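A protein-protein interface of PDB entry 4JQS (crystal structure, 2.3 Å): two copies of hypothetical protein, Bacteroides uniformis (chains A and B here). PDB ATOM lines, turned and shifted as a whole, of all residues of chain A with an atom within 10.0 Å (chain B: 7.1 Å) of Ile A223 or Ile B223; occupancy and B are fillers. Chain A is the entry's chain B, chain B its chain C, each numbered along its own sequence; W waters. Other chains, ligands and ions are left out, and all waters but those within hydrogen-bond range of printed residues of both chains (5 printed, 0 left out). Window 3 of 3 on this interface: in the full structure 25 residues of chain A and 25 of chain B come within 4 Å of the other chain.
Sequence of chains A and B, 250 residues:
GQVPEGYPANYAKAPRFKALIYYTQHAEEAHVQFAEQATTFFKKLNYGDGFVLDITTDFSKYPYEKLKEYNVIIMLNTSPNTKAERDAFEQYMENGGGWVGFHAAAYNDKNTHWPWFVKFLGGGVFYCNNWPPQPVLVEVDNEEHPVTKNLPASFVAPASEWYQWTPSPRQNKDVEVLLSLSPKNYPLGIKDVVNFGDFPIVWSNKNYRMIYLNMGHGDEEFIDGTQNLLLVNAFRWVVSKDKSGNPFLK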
ATOM      1  N   PHE A  34      14.971 -16.827 -23.033  1.00  0.00           N
ATOM      2  CA  PHE A  34      14.995 -15.771 -24.038  1.00  0.00           C
ATOM      3  C   PHE A  34      14.370 -16.288 -25.343  1.00  0.00           C
ATOM      4  O   PHE A  34      13.466 -15.641 -25.887  1.00  0.00           O
ATOM      5  CB  PHE A  34      16.418 -15.219 -24.291  1.00  0.00           C
ATOM      6  CG  PHE A  34      16.433 -14.341 -25.528  1.00  0.00           C
ATOM      7  CD1 PHE A  34      15.777 -13.107 -25.536  1.00  0.00           C
ATOM      8  CD2 PHE A  34      17.009 -14.791 -26.715  1.00  0.00           C
ATOM      9  CE1 PHE A  34      15.743 -12.323 -26.702  1.00  0.00           C
ATOM     10  CE2 PHE A  34      16.954 -14.017 -27.879  1.00  0.00           C
ATOM     11  CZ  PHE A  34      16.328 -12.789 -27.864  1.00  0.00           C
ATOM     12  N   GLN A  37      10.528 -16.571 -25.168  1.00  0.00           N
ATOM     13  CA  GLN A  37       9.885 -15.243 -25.176  1.00  0.00           C
ATOM     14  C   GLN A  37      10.055 -14.556 -26.539  1.00  0.00           C
ATOM     15  O   GLN A  37       9.144 -13.848 -26.981  1.00  0.00           O
ATOM     16  CB  GLN A  37      10.457 -14.328 -24.076  1.00  0.00           C
ATOM     17  CG  GLN A  37       9.961 -14.655 -22.672  1.00  0.00           C
ATOM     18  CD  GLN A  37      10.249 -13.554 -21.669  1.00  0.00           C
ATOM     19  OE1 GLN A  37      10.967 -12.560 -21.923  1.00  0.00           O
ATOM     20  NE2 GLN A  37       9.648 -13.693 -20.502  1.00  0.00           N
ATOM     21  N   PHE A  41       7.292 -13.175 -29.286  1.00  0.00           N
ATOM     22  CA  PHE A  41       7.453 -11.844 -29.877  1.00  0.00           C
ATOM     23  C   PHE A  41       7.253 -11.918 -31.418  1.00  0.00           C
ATOM     24  O   PHE A  41       6.444 -11.168 -31.947  1.00  0.00           O
ATOM     25  CB  PHE A  41       8.825 -11.262 -29.504  1.00  0.00           C
ATOM     26  CG  PHE A  41       9.211  -9.957 -30.182  1.00  0.00           C
ATOM     27  CD1 PHE A  41       8.750  -8.737 -29.693  1.00  0.00           C
ATOM     28  CD2 PHE A  41      10.063  -9.950 -31.276  1.00  0.00           C
ATOM     29  CE1 PHE A  41       9.108  -7.538 -30.308  1.00  0.00           C
ATOM     30  CE2 PHE A  41      10.421  -8.751 -31.899  1.00  0.00           C
ATOM     31  CZ  PHE A  41       9.943  -7.554 -31.408  1.00  0.00           C
ATOM     32  N   GLN A 134      22.761  -7.172 -16.667  1.00  0.00           N
ATOM     33  CA  GLN A 134      22.290  -5.891 -16.160  1.00  0.00           C
ATOM     34  C   GLN A 134      21.940  -4.951 -17.300  1.00  0.00           C
ATOM     35  O   GLN A 134      22.438  -5.137 -18.411  1.00  0.00           O
ATOM     36  CB  GLN A 134      23.351  -5.242 -15.244  1.00  0.00           C
ATOM     37  CG  GLN A 134      24.653  -4.853 -15.957  1.00  0.00           C
ATOM     38  CD  GLN A 134      25.361  -3.809 -15.150  1.00  0.00           C
ATOM     39  OE1 GLN A 134      26.181  -4.114 -14.272  1.00  0.00           O
ATOM     40  NE2 GLN A 134      25.071  -2.552 -15.445  1.00  0.00           N
ATOM     41  N   PRO A 135      21.103  -3.907 -17.050  1.00  0.00           N
ATOM     42  CA  PRO A 135      20.873  -2.908 -18.108  1.00  0.00           C
ATOM     43  C   PRO A 135      22.161  -2.128 -18.379  1.00  0.00           C
ATOM     44  O   PRO A 135      23.026  -2.059 -17.505  1.00  0.00           O
ATOM     45  CB  PRO A 135      19.791  -1.993 -17.510  1.00  0.00           C
ATOM     46  CG  PRO A 135      19.349  -2.631 -16.236  1.00  0.00           C
ATOM     47  CD  PRO A 135      20.448  -3.506 -15.783  1.00  0.00           C
ATOM     48  N   VAL A 156      18.975   3.243 -22.533  1.00  0.00           N
ATOM     49  CA  VAL A 156      19.354   2.166 -21.643  1.00  0.00           C
ATOM     50  C   VAL A 156      18.643   0.906 -22.125  1.00  0.00           C
ATOM     51  O   VAL A 156      17.415   0.837 -22.090  1.00  0.00           O
ATOM     52  CB  VAL A 156      19.059   2.505 -20.154  1.00  0.00           C
ATOM     53  CG1 VAL A 156      19.230   1.275 -19.252  1.00  0.00           C
ATOM     54  CG2 VAL A 156      19.948   3.650 -19.675  1.00  0.00           C
ATOM     55  N   ALA A 157      19.421  -0.095 -22.565  1.00  0.00           N
ATOM     56  CA  ALA A 157      18.864  -1.387 -22.985  1.00  0.00           C
ATOM     57  C   ALA A 157      18.485  -2.194 -21.740  1.00  0.00           C
ATOM     58  O   ALA A 157      19.206  -2.080 -20.748  1.00  0.00           O
ATOM     59  CB  ALA A 157      19.892  -2.157 -23.827  1.00  0.00           C
ATOM     60  N   PRO A 158      17.424  -3.045 -21.731  1.00  0.00           N
ATOM     61  CA  PRO A 158      17.167  -3.871 -20.523  1.00  0.00           C
ATOM     62  C   PRO A 158      18.297  -4.909 -20.276  1.00  0.00           C
ATOM     63  O   PRO A 158      19.187  -5.123 -21.120  1.00  0.00           O
ATOM     64  CB  PRO A 158      15.815  -4.538 -20.826  1.00  0.00           C
ATOM     65  CG  PRO A 158      15.706  -4.551 -22.295  1.00  0.00           C
ATOM     66  CD  PRO A 158      16.455  -3.346 -22.808  1.00  0.00           C
ATOM     67  N   ALA A 159      18.269  -5.538 -19.103  1.00  0.00           N
ATOM     68  CA  ALA A 159      19.267  -6.498 -18.646  1.00  0.00           C
ATOM     69  C   ALA A 159      19.577  -7.631 -19.624  1.00  0.00           C
ATOM     70  O   ALA A 159      18.679  -8.306 -20.145  1.00  0.00           O
ATOM     71  CB  ALA A 159      18.852  -7.096 -17.307  1.00  0.00           C
ATOM     72  N   SER A 160      20.890  -7.845 -19.828  1.00  0.00           N
ATOM     73  CA  SER A 160      21.486  -8.945 -20.558  1.00  0.00           C
ATOM     74  C   SER A 160      22.919  -9.130 -20.103  1.00  0.00           C
ATOM     75  O   SER A 160      23.505  -8.261 -19.468  1.00  0.00           O
ATOM     76  CB  SER A 160      21.437  -8.720 -22.074  1.00  0.00           C
ATOM     77  OG  SER A 160      21.882  -9.870 -22.786  1.00  0.00           O
ATOM     78  N   HIS A 217      19.276 -12.802 -23.286  1.00  0.00           N
ATOM     79  CA  HIS A 217      19.513 -13.548 -22.062  1.00  0.00           C
ATOM     80  C   HIS A 217      18.437 -13.252 -21.030  1.00  0.00           C
ATOM     81  O   HIS A 217      18.213 -12.085 -20.701  1.00  0.00           O
ATOM     82  CB  HIS A 217      20.910 -13.144 -21.515  1.00  0.00           C
ATOM     83  CG  HIS A 217      21.382 -13.929 -20.329  1.00  0.00           C
ATOM     84  ND1 HIS A 217      22.372 -14.897 -20.453  1.00  0.00           N
ATOM     85  CD2 HIS A 217      20.989 -13.863 -19.032  1.00  0.00           C
ATOM     86  CE1 HIS A 217      22.555 -15.376 -19.234  1.00  0.00           C
ATOM     87  NE2 HIS A 217      21.754 -14.779 -18.344  1.00  0.00           N
ATOM     88  N   GLY A 218      17.841 -14.313 -20.486  1.00  0.00           N
ATOM     89  CA  GLY A 218      16.864 -14.224 -19.410  1.00  0.00           C
ATOM     90  C   GLY A 218      15.416 -14.040 -19.831  1.00  0.00           C
ATOM     91  O   GLY A 218      15.072 -14.143 -21.017  1.00  0.00           O
ATOM     92  N   ASP A 219      14.561 -13.721 -18.845  1.00  0.00           N
ATOM     93  CA  ASP A 219      13.128 -13.590 -19.086  1.00  0.00           C
ATOM     94  C   ASP A 219      12.615 -12.120 -19.042  1.00  0.00           C
ATOM     95  O   ASP A 219      11.416 -11.904 -18.842  1.00  0.00           O
ATOM     96  CB  ASP A 219      12.363 -14.474 -18.085  1.00  0.00           C
ATOM     97  CG  ASP A 219      12.541 -14.107 -16.608  1.00  0.00           C
ATOM     98  OD1 ASP A 219      13.443 -13.290 -16.297  1.00  0.00           O
ATOM     99  OD2 ASP A 219      11.783 -14.651 -15.765  1.00  0.00           O
ATOM    100  N   GLU A 220      13.489 -11.121 -19.268  1.00  0.00           N
ATOM    101  CA  GLU A 220      13.025  -9.729 -19.224  1.00  0.00           C
ATOM    102  C   GLU A 220      13.531  -8.882 -20.405  1.00  0.00           C
ATOM    103  O   GLU A 220      13.660  -7.657 -20.279  1.00  0.00           O
ATOM    104  CB  GLU A 220      13.430  -9.072 -17.894  1.00  0.00           C
ATOM    105  CG  GLU A 220      12.553  -9.470 -16.719  1.00  0.00           C
ATOM    106  CD  GLU A 220      12.887  -8.841 -15.377  1.00  0.00           C
ATOM    107  OE1 GLU A 220      13.764  -7.947 -15.316  1.00  0.00           O
ATOM    108  OE2 GLU A 220      12.279  -9.277 -14.372  1.00  0.00           O
ATOM    109  N   GLU A 221      13.786  -9.508 -21.558  1.00  0.00           N
ATOM    110  CA  GLU A 221      14.303  -8.783 -22.712  1.00  0.00           C
ATOM    111  C   GLU A 221      13.222  -8.045 -23.529  1.00  0.00           C
ATOM    112  O   GLU A 221      13.572  -7.347 -24.494  1.00  0.00           O
ATOM    113  CB  GLU A 221      15.069  -9.755 -23.614  1.00  0.00           C
ATOM    114  CG  GLU A 221      16.299 -10.333 -22.927  1.00  0.00           C
ATOM    115  CD  GLU A 221      17.571  -9.529 -23.090  1.00  0.00           C
ATOM    116  OE1 GLU A 221      17.470  -8.298 -23.271  1.00  0.00           O
ATOM    117  OE2 GLU A 221      18.669 -10.126 -23.058  1.00  0.00           O
ATOM    118  N   PHE A 222      11.923  -8.164 -23.132  1.00  0.00           N
ATOM    119  CA  PHE A 222      10.808  -7.547 -23.879  1.00  0.00           C
ATOM    120  C   PHE A 222      10.038  -6.507 -23.054  1.00  0.00           C
ATOM    121  O   PHE A 222       8.957  -6.078 -23.460  1.00  0.00           O
ATOM    122  CB  PHE A 222       9.879  -8.647 -24.459  1.00  0.00           C
ATOM    123  CG  PHE A 222      10.629  -9.445 -25.517  1.00  0.00           C
ATOM    124  CD1 PHE A 222      10.815  -8.932 -26.798  1.00  0.00           C
ATOM    125  CD2 PHE A 222      11.275 -10.638 -25.190  1.00  0.00           C
ATOM    126  CE1 PHE A 222      11.592  -9.625 -27.740  1.00  0.00           C
ATOM    127  CE2 PHE A 222      12.052 -11.323 -26.134  1.00  0.00           C
ATOM    128  CZ  PHE A 222      12.209 -10.809 -27.399  1.00  0.00           C
ATOM    129  N   ILE A 223      10.639  -6.049 -21.949  1.00  0.00           N
ATOM    130  CA  ILE A 223      10.044  -5.051 -21.027  1.00  0.00           C
ATOM    131  C   ILE A 223      10.207  -3.590 -21.561  1.00  0.00           C
ATOM    132  O   ILE A 223       9.599  -2.667 -21.014  1.00  0.00           O
ATOM    133  CB  ILE A 223      10.645  -5.174 -19.575  1.00  0.00           C
ATOM    134  CG1 ILE A 223      12.158  -4.808 -19.527  1.00  0.00           C
ATOM    135  CG2 ILE A 223      10.358  -6.544 -18.967  1.00  0.00           C
ATOM    136  CD1 ILE A 223      12.737  -4.344 -18.073  1.00  0.00           C
ATOM    137  N   ASP A 224      11.034  -3.400 -22.589  1.00  0.00           N
ATOM    138  CA  ASP A 224      11.386  -2.087 -23.106  1.00  0.00           C
ATOM    139  C   ASP A 224      10.957  -1.859 -24.571  1.00  0.00           C
ATOM    140  O   ASP A 224      11.402  -2.572 -25.471  1.00  0.00           O
ATOM    141  CB  ASP A 224      12.909  -1.899 -22.969  1.00  0.00           C
ATOM    142  CG  ASP A 224      13.352  -0.495 -23.183  1.00  0.00           C
ATOM    143  OD1 ASP A 224      13.025   0.370 -22.324  1.00  0.00           O
ATOM    144  OD2 ASP A 224      14.015  -0.240 -24.208  1.00  0.00           O
ATOM    145  N   GLY A 225      10.136  -0.830 -24.785  1.00  0.00           N
ATOM    146  CA  GLY A 225       9.660  -0.445 -26.113  1.00  0.00           C
ATOM    147  C   GLY A 225      10.773  -0.103 -27.090  1.00  0.00           C
ATOM    148  O   GLY A 225      10.697  -0.507 -28.249  1.00  0.00           O
ATOM    149  N   THR A 226      11.832   0.627 -26.627  1.00  0.00           N
ATOM    150  CA  THR A 226      12.960   1.017 -27.479  1.00  0.00           C
ATOM    151  C   THR A 226      13.731  -0.223 -28.004  1.00  0.00           C
ATOM    152  O   THR A 226      13.984  -0.309 -29.205  1.00  0.00           O
ATOM    153  CB  THR A 226      13.907   1.991 -26.763  1.00  0.00           C
ATOM    154  OG1 THR A 226      13.153   3.051 -26.195  1.00  0.00           O
ATOM    155  CG2 THR A 226      14.958   2.564 -27.694  1.00  0.00           C
ATOM    156  N   GLN A 227      14.076  -1.179 -27.125  1.00  0.00           N
ATOM    157  CA  GLN A 227      14.766  -2.376 -27.583  1.00  0.00           C
ATOM    158  C   GLN A 227      13.829  -3.254 -28.462  1.00  0.00           C
ATOM    159  O   GLN A 227      14.301  -3.887 -29.404  1.00  0.00           O
ATOM    160  CB  GLN A 227      15.352  -3.184 -26.413  1.00  0.00           C
ATOM    161  CG  GLN A 227      16.289  -4.276 -26.929  1.00  0.00           C
ATOM    162  CD  GLN A 227      16.805  -5.181 -25.864  1.00  0.00           C
ATOM    163  OE1 GLN A 227      17.907  -4.987 -25.352  1.00  0.00           O
ATOM    164  NE2 GLN A 227      16.068  -6.242 -25.577  1.00  0.00           N
ATOM    165  N   ASN A 228      12.506  -3.256 -28.182  1.00  0.00           N
ATOM    166  CA  ASN A 228      11.582  -4.033 -28.994  1.00  0.00           C
ATOM    167  C   ASN A 228      11.524  -3.472 -30.416  1.00  0.00           C
ATOM    168  O   ASN A 228      11.445  -4.250 -31.370  1.00  0.00           O
ATOM    169  CB  ASN A 228      10.194  -4.087 -28.360  1.00  0.00           C
ATOM    170  CG  ASN A 228      10.135  -4.868 -27.059  1.00  0.00           C
ATOM    171  OD1 ASN A 228      11.097  -5.514 -26.629  1.00  0.00           O
ATOM    172  ND2 ASN A 228       9.037  -4.736 -26.343  1.00  0.00           N
ATOM    173  N   LEU A 229      11.616  -2.126 -30.554  1.00  0.00           N
ATOM    174  CA  LEU A 229      11.628  -1.440 -31.845  1.00  0.00           C
ATOM    175  C   LEU A 229      12.904  -1.836 -32.614  1.00  0.00           C
ATOM    176  O   LEU A 229      12.798  -2.199 -33.768  1.00  0.00           O
ATOM    177  CB  LEU A 229      11.504   0.106 -31.675  1.00  0.00           C
ATOM    178  CG  LEU A 229      11.414   0.920 -32.992  1.00  0.00           C
ATOM    179  CD1 LEU A 229      10.300   0.427 -33.885  1.00  0.00           C
ATOM    180  CD2 LEU A 229      11.248   2.401 -32.739  1.00  0.00           C
ATOM    181  N   LEU A 231      14.557  -4.620 -32.450  1.00  0.00           N
ATOM    182  CA  LEU A 231      14.319  -6.001 -32.906  1.00  0.00           C
ATOM    183  C   LEU A 231      13.391  -6.036 -34.123  1.00  0.00           C
ATOM    184  O   LEU A 231      13.689  -6.757 -35.075  1.00  0.00           O
ATOM    185  CB  LEU A 231      13.782  -6.891 -31.767  1.00  0.00           C
ATOM    186  CG  LEU A 231      14.825  -7.708 -31.021  1.00  0.00           C
ATOM    187  CD1 LEU A 231      15.794  -6.818 -30.211  1.00  0.00           C
ATOM    188  CD2 LEU A 231      14.160  -8.774 -30.129  1.00  0.00           C
ATOM    189  N   GLN B  37       9.815  -7.589  -4.251  1.00  0.00           N
ATOM    190  CA  GLN B  37      10.309  -7.499  -5.633  1.00  0.00           C
ATOM    191  C   GLN B  37      11.770  -7.029  -5.679  1.00  0.00           C
ATOM    192  O   GLN B  37      12.526  -7.483  -6.541  1.00  0.00           O
ATOM    193  CB  GLN B  37       9.453  -6.540  -6.478  1.00  0.00           C
ATOM    194  CG  GLN B  37       8.124  -7.132  -6.911  1.00  0.00           C
ATOM    195  CD  GLN B  37       7.464  -6.379  -8.047  1.00  0.00           C
ATOM    196  OE1 GLN B  37       7.882  -5.275  -8.478  1.00  0.00           O
ATOM    197  NE2 GLN B  37       6.408  -6.987  -8.572  1.00  0.00           N
ATOM    198  N   PRO B 158       9.501   5.012 -13.338  1.00  0.00           N
ATOM    199  CA  PRO B 158       8.166   4.381 -13.206  1.00  0.00           C
ATOM    200  C   PRO B 158       7.442   4.841 -11.910  1.00  0.00           C
ATOM    201  O   PRO B 158       8.033   5.503 -11.043  1.00  0.00           O
ATOM    202  CB  PRO B 158       8.473   2.873 -13.209  1.00  0.00           C
ATOM    203  CG  PRO B 158       9.875   2.764 -12.736  1.00  0.00           C
ATOM    204  CD  PRO B 158      10.588   4.015 -13.195  1.00  0.00           C
ATOM    205  N   ALA B 159       6.155   4.506 -11.798  1.00  0.00           N
ATOM    206  CA  ALA B 159       5.283   4.918 -10.693  1.00  0.00           C
ATOM    207  C   ALA B 159       5.839   4.641  -9.295  1.00  0.00           C
ATOM    208  O   ALA B 159       6.327   3.544  -8.997  1.00  0.00           O
ATOM    209  CB  ALA B 159       3.907   4.275 -10.825  1.00  0.00           C
ATOM    210  N   ASP B 219       4.118  -2.640  -6.870  1.00  0.00           N
ATOM    211  CA  ASP B 219       4.581  -3.841  -7.557  1.00  0.00           C
ATOM    212  C   ASP B 219       5.030  -3.595  -9.030  1.00  0.00           C
ATOM    213  O   ASP B 219       5.108  -4.552  -9.805  1.00  0.00           O
ATOM    214  CB  ASP B 219       3.476  -4.923  -7.493  1.00  0.00           C
ATOM    215  CG  ASP B 219       2.162  -4.564  -8.195  1.00  0.00           C
ATOM    216  OD1 ASP B 219       1.983  -3.370  -8.571  1.00  0.00           O
ATOM    217  OD2 ASP B 219       1.328  -5.469  -8.384  1.00  0.00           O
ATOM    218  N   GLU B 220       5.390  -2.369  -9.397  1.00  0.00           N
ATOM    219  CA  GLU B 220       5.826  -2.153 -10.791  1.00  0.00           C
ATOM    220  C   GLU B 220       7.089  -1.251 -10.862  1.00  0.00           C
ATOM    221  O   GLU B 220       7.310  -0.547 -11.850  1.00  0.00           O
ATOM    222  CB  GLU B 220       4.683  -1.645 -11.728  1.00  0.00           C
ATOM    223  CG  GLU B 220       3.648  -0.676 -11.165  1.00  0.00           C
ATOM    224  CD  GLU B 220       3.202   0.492 -12.044  1.00  0.00           C
ATOM    225  OE1 GLU B 220       4.041   1.030 -12.809  1.00  0.00           O
ATOM    226  OE2 GLU B 220       2.034   0.926 -11.895  1.00  0.00           O
ATOM    227  N   GLU B 221       7.955  -1.354  -9.836  1.00  0.00           N
ATOM    228  CA  GLU B 221       9.175  -0.557  -9.764  1.00  0.00           C
ATOM    229  C   GLU B 221      10.317  -1.110 -10.607  1.00  0.00           C
ATOM    230  O   GLU B 221      11.345  -0.443 -10.701  1.00  0.00           O
ATOM    231  CB  GLU B 221       9.637  -0.432  -8.309  1.00  0.00           C
ATOM    232  CG  GLU B 221       8.727   0.438  -7.472  1.00  0.00           C
ATOM    233  CD  GLU B 221       9.027   1.921  -7.538  1.00  0.00           C
ATOM    234  OE1 GLU B 221       9.457   2.411  -8.608  1.00  0.00           O
ATOM    235  OE2 GLU B 221       8.818   2.599  -6.511  1.00  0.00           O
ATOM    236  N   PHE B 222      10.153  -2.296 -11.232  1.00  0.00           N
ATOM    237  CA  PHE B 222      11.228  -2.947 -11.998  1.00  0.00           C
ATOM    238  C   PHE B 222      10.890  -3.127 -13.496  1.00  0.00           C
ATOM    239  O   PHE B 222      11.578  -3.856 -14.199  1.00  0.00           O
ATOM    240  CB  PHE B 222      11.602  -4.281 -11.318  1.00  0.00           C
ATOM    241  CG  PHE B 222      12.239  -4.018  -9.966  1.00  0.00           C
ATOM    242  CD1 PHE B 222      13.569  -3.626  -9.874  1.00  0.00           C
ATOM    243  CD2 PHE B 222      11.478  -4.048  -8.800  1.00  0.00           C
ATOM    244  CE1 PHE B 222      14.135  -3.308  -8.636  1.00  0.00           C
ATOM    245  CE2 PHE B 222      12.043  -3.715  -7.563  1.00  0.00           C
ATOM    246  CZ  PHE B 222      13.367  -3.345  -7.490  1.00  0.00           C
ATOM    247  N   ILE B 223       9.890  -2.385 -13.981  1.00  0.00           N
ATOM    248  CA  ILE B 223       9.434  -2.421 -15.378  1.00  0.00           C
ATOM    249  C   ILE B 223      10.338  -1.566 -16.317  1.00  0.00           C
ATOM    250  O   ILE B 223      10.207  -1.662 -17.537  1.00  0.00           O
ATOM    251  CB  ILE B 223       7.934  -1.960 -15.498  1.00  0.00           C
ATOM    252  CG1 ILE B 223       7.731  -0.449 -15.131  1.00  0.00           C
ATOM    253  CG2 ILE B 223       6.995  -2.906 -14.730  1.00  0.00           C
ATOM    254  CD1 ILE B 223       6.436   0.248 -15.737  1.00  0.00           C
ATOM    255  N   ASP B 224      11.216  -0.731 -15.745  1.00  0.00           N
ATOM    256  CA  ASP B 224      12.037   0.207 -16.483  1.00  0.00           C
ATOM    257  C   ASP B 224      13.541  -0.068 -16.381  1.00  0.00           C
ATOM    258  O   ASP B 224      14.113  -0.026 -15.287  1.00  0.00           O
ATOM    259  CB  ASP B 224      11.732   1.619 -15.962  1.00  0.00           C
ATOM    260  CG  ASP B 224      12.251   2.713 -16.863  1.00  0.00           C
ATOM    261  OD1 ASP B 224      11.714   2.856 -17.986  1.00  0.00           O
ATOM    262  OD2 ASP B 224      13.205   3.421 -16.453  1.00  0.00           O
ATOM    263  N   GLY B 225      14.171  -0.275 -17.540  1.00  0.00           N
ATOM    264  CA  GLY B 225      15.613  -0.493 -17.664  1.00  0.00           C
ATOM    265  C   GLY B 225      16.462   0.634 -17.092  1.00  0.00           C
ATOM    266  O   GLY B 225      17.448   0.367 -16.402  1.00  0.00           O
ATOM    267  N   THR B 226      16.079   1.900 -17.341  1.00  0.00           N
ATOM    268  CA  THR B 226      16.820   3.077 -16.860  1.00  0.00           C
ATOM    269  C   THR B 226      16.836   3.139 -15.319  1.00  0.00           C
ATOM    270  O   THR B 226      17.910   3.323 -14.740  1.00  0.00           O
ATOM    271  CB  THR B 226      16.269   4.384 -17.457  1.00  0.00           C
ATOM    272  OG1 THR B 226      16.132   4.249 -18.876  1.00  0.00           O
ATOM    273  CG2 THR B 226      17.139   5.585 -17.115  1.00  0.00           C
ATOM    274  N   GLN B 227      15.664   2.970 -14.658  1.00  0.00           N
ATOM    275  CA  GLN B 227      15.642   2.989 -13.199  1.00  0.00           C
ATOM    276  C   GLN B 227      16.365   1.742 -12.625  1.00  0.00           C
ATOM    277  O   GLN B 227      17.002   1.848 -11.568  1.00  0.00           O
ATOM    278  CB  GLN B 227      14.216   3.100 -12.648  1.00  0.00           C
ATOM    279  CG  GLN B 227      14.255   3.384 -11.137  1.00  0.00           C
ATOM    280  CD  GLN B 227      12.916   3.436 -10.506  1.00  0.00           C
ATOM    281  OE1 GLN B 227      12.333   4.506 -10.391  1.00  0.00           O
ATOM    282  NE2 GLN B 227      12.410   2.283 -10.079  1.00  0.00           N
ATOM    283  N   ASN B 228      16.308   0.585 -13.333  1.00  0.00           N
ATOM    284  CA  ASN B 228      16.994  -0.615 -12.852  1.00  0.00           C
ATOM    285  C   ASN B 228      18.498  -0.397 -12.871  1.00  0.00           C
ATOM    286  O   ASN B 228      19.177  -0.845 -11.947  1.00  0.00           O
ATOM    287  CB  ASN B 228      16.596  -1.852 -13.658  1.00  0.00           C
ATOM    288  CG  ASN B 228      15.144  -2.282 -13.467  1.00  0.00           C
ATOM    289  OD1 ASN B 228      14.398  -1.755 -12.632  1.00  0.00           O
ATOM    290  ND2 ASN B 228      14.676  -3.182 -14.318  1.00  0.00           N
HETATM  291  O   HOH W   1      16.480  -4.451 -16.926  1.00  0.00           O
HETATM  292  O   HOH W   2      15.158   0.912 -20.622  1.00  0.00           O
HETATM  293  O   HOH W   3       9.756  -0.497 -19.688  1.00  0.00           O
HETATM  294  O   HOH W   4      12.293  -0.441 -19.911  1.00  0.00           O
HETATM  295  O   HOH W   5      16.868   4.984 -21.510  1.00  0.00           O
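Water W3 bridges O of Ile B223 (2.5 Å) and O of Ile A223 (2.5 Å).
Water W4 lies within hydrogen-bond range of OD1 of Asp A224 (2.6 Å), N of Gly B225 (3.0 Å) and O of Ile B223 (3.4 Å).
Water W2 lies within hydrogen-bond range of O of Val A156 (2.7 Å), OD1 of Asp A224 (2.8 Å) and N of Gly B225 (3.4 Å).
Water W5 lies within hydrogen-bond range of the side-chain hydroxyl of Thr B226 (2.8 Å) and the backbone NH of Val A156 (2.9 Å).
Water W1 bridges the backbone NH (N) of Ala A159 (3.0 Å) and the side-chain amide nitrogen (ND2) of Asn B228 (3.4 Å).
Ile A223 touches its own counterpart, Ile B223.
Of the 5 pairs that touch across the chains among the printed residues, 1 has its exchanged pair printed and touching as well.
Of the printed residues of chain B, Pro A135 touches Gly B225 (3.5 Å) and Asn B228 (3.9 Å).
His A217 touches none of the printed residues of chain B.
Of chain B, only Ile B223 comes within 4 Å of Ile A223.
Leu A231 touches none of the printed residues of chain B.
No residue of chain A comes within 4 Å of Glu B220.
Ile B223 touches one residue of chain A.
Asp B224 touches none of the printed residues of chain A.
Printed residues of chain A within 4 Å of Gly B225: Pro A135 (3.5 Å) and Val A156 (3.5 Å).
Printed residues of chain A within 4 Å of Thr B226: Val A156 (3.6 Å).
Of the printed residues of chain A, Asn B228 touches Pro A135.
The nearest residue of chain B that does not touch Ile A223 is Phe B222 (4.1 Å).
The nearest residue of chain A that does not touch Ile B223 is Asp A224 (5.4 Å).
Among the printed residues, merely in contact across the chains: Val A156 with Gly B225 (3.5 Å), Pro A135 with Gly B225 (3.5 Å), Val A156 with Thr B226 (3.6 Å), Ile A223 with Ile B223 (3.7 Å) and Pro A135 with Asn B228 (3.9 Å).
The backbone carbonyl oxygen (O) of Phe B222 is in hydrogen-bond range of the side-chain amide nitrogen (ND2) of Asn B228 (3.2 Å).
OD1 of Asn B228 lies close to O of Asp B224 (3.2 Å).
The side-chain carboxylate (OD2) of Asp B224 sits close to the backbone NH (N) of Thr B226 (3.4 Å).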
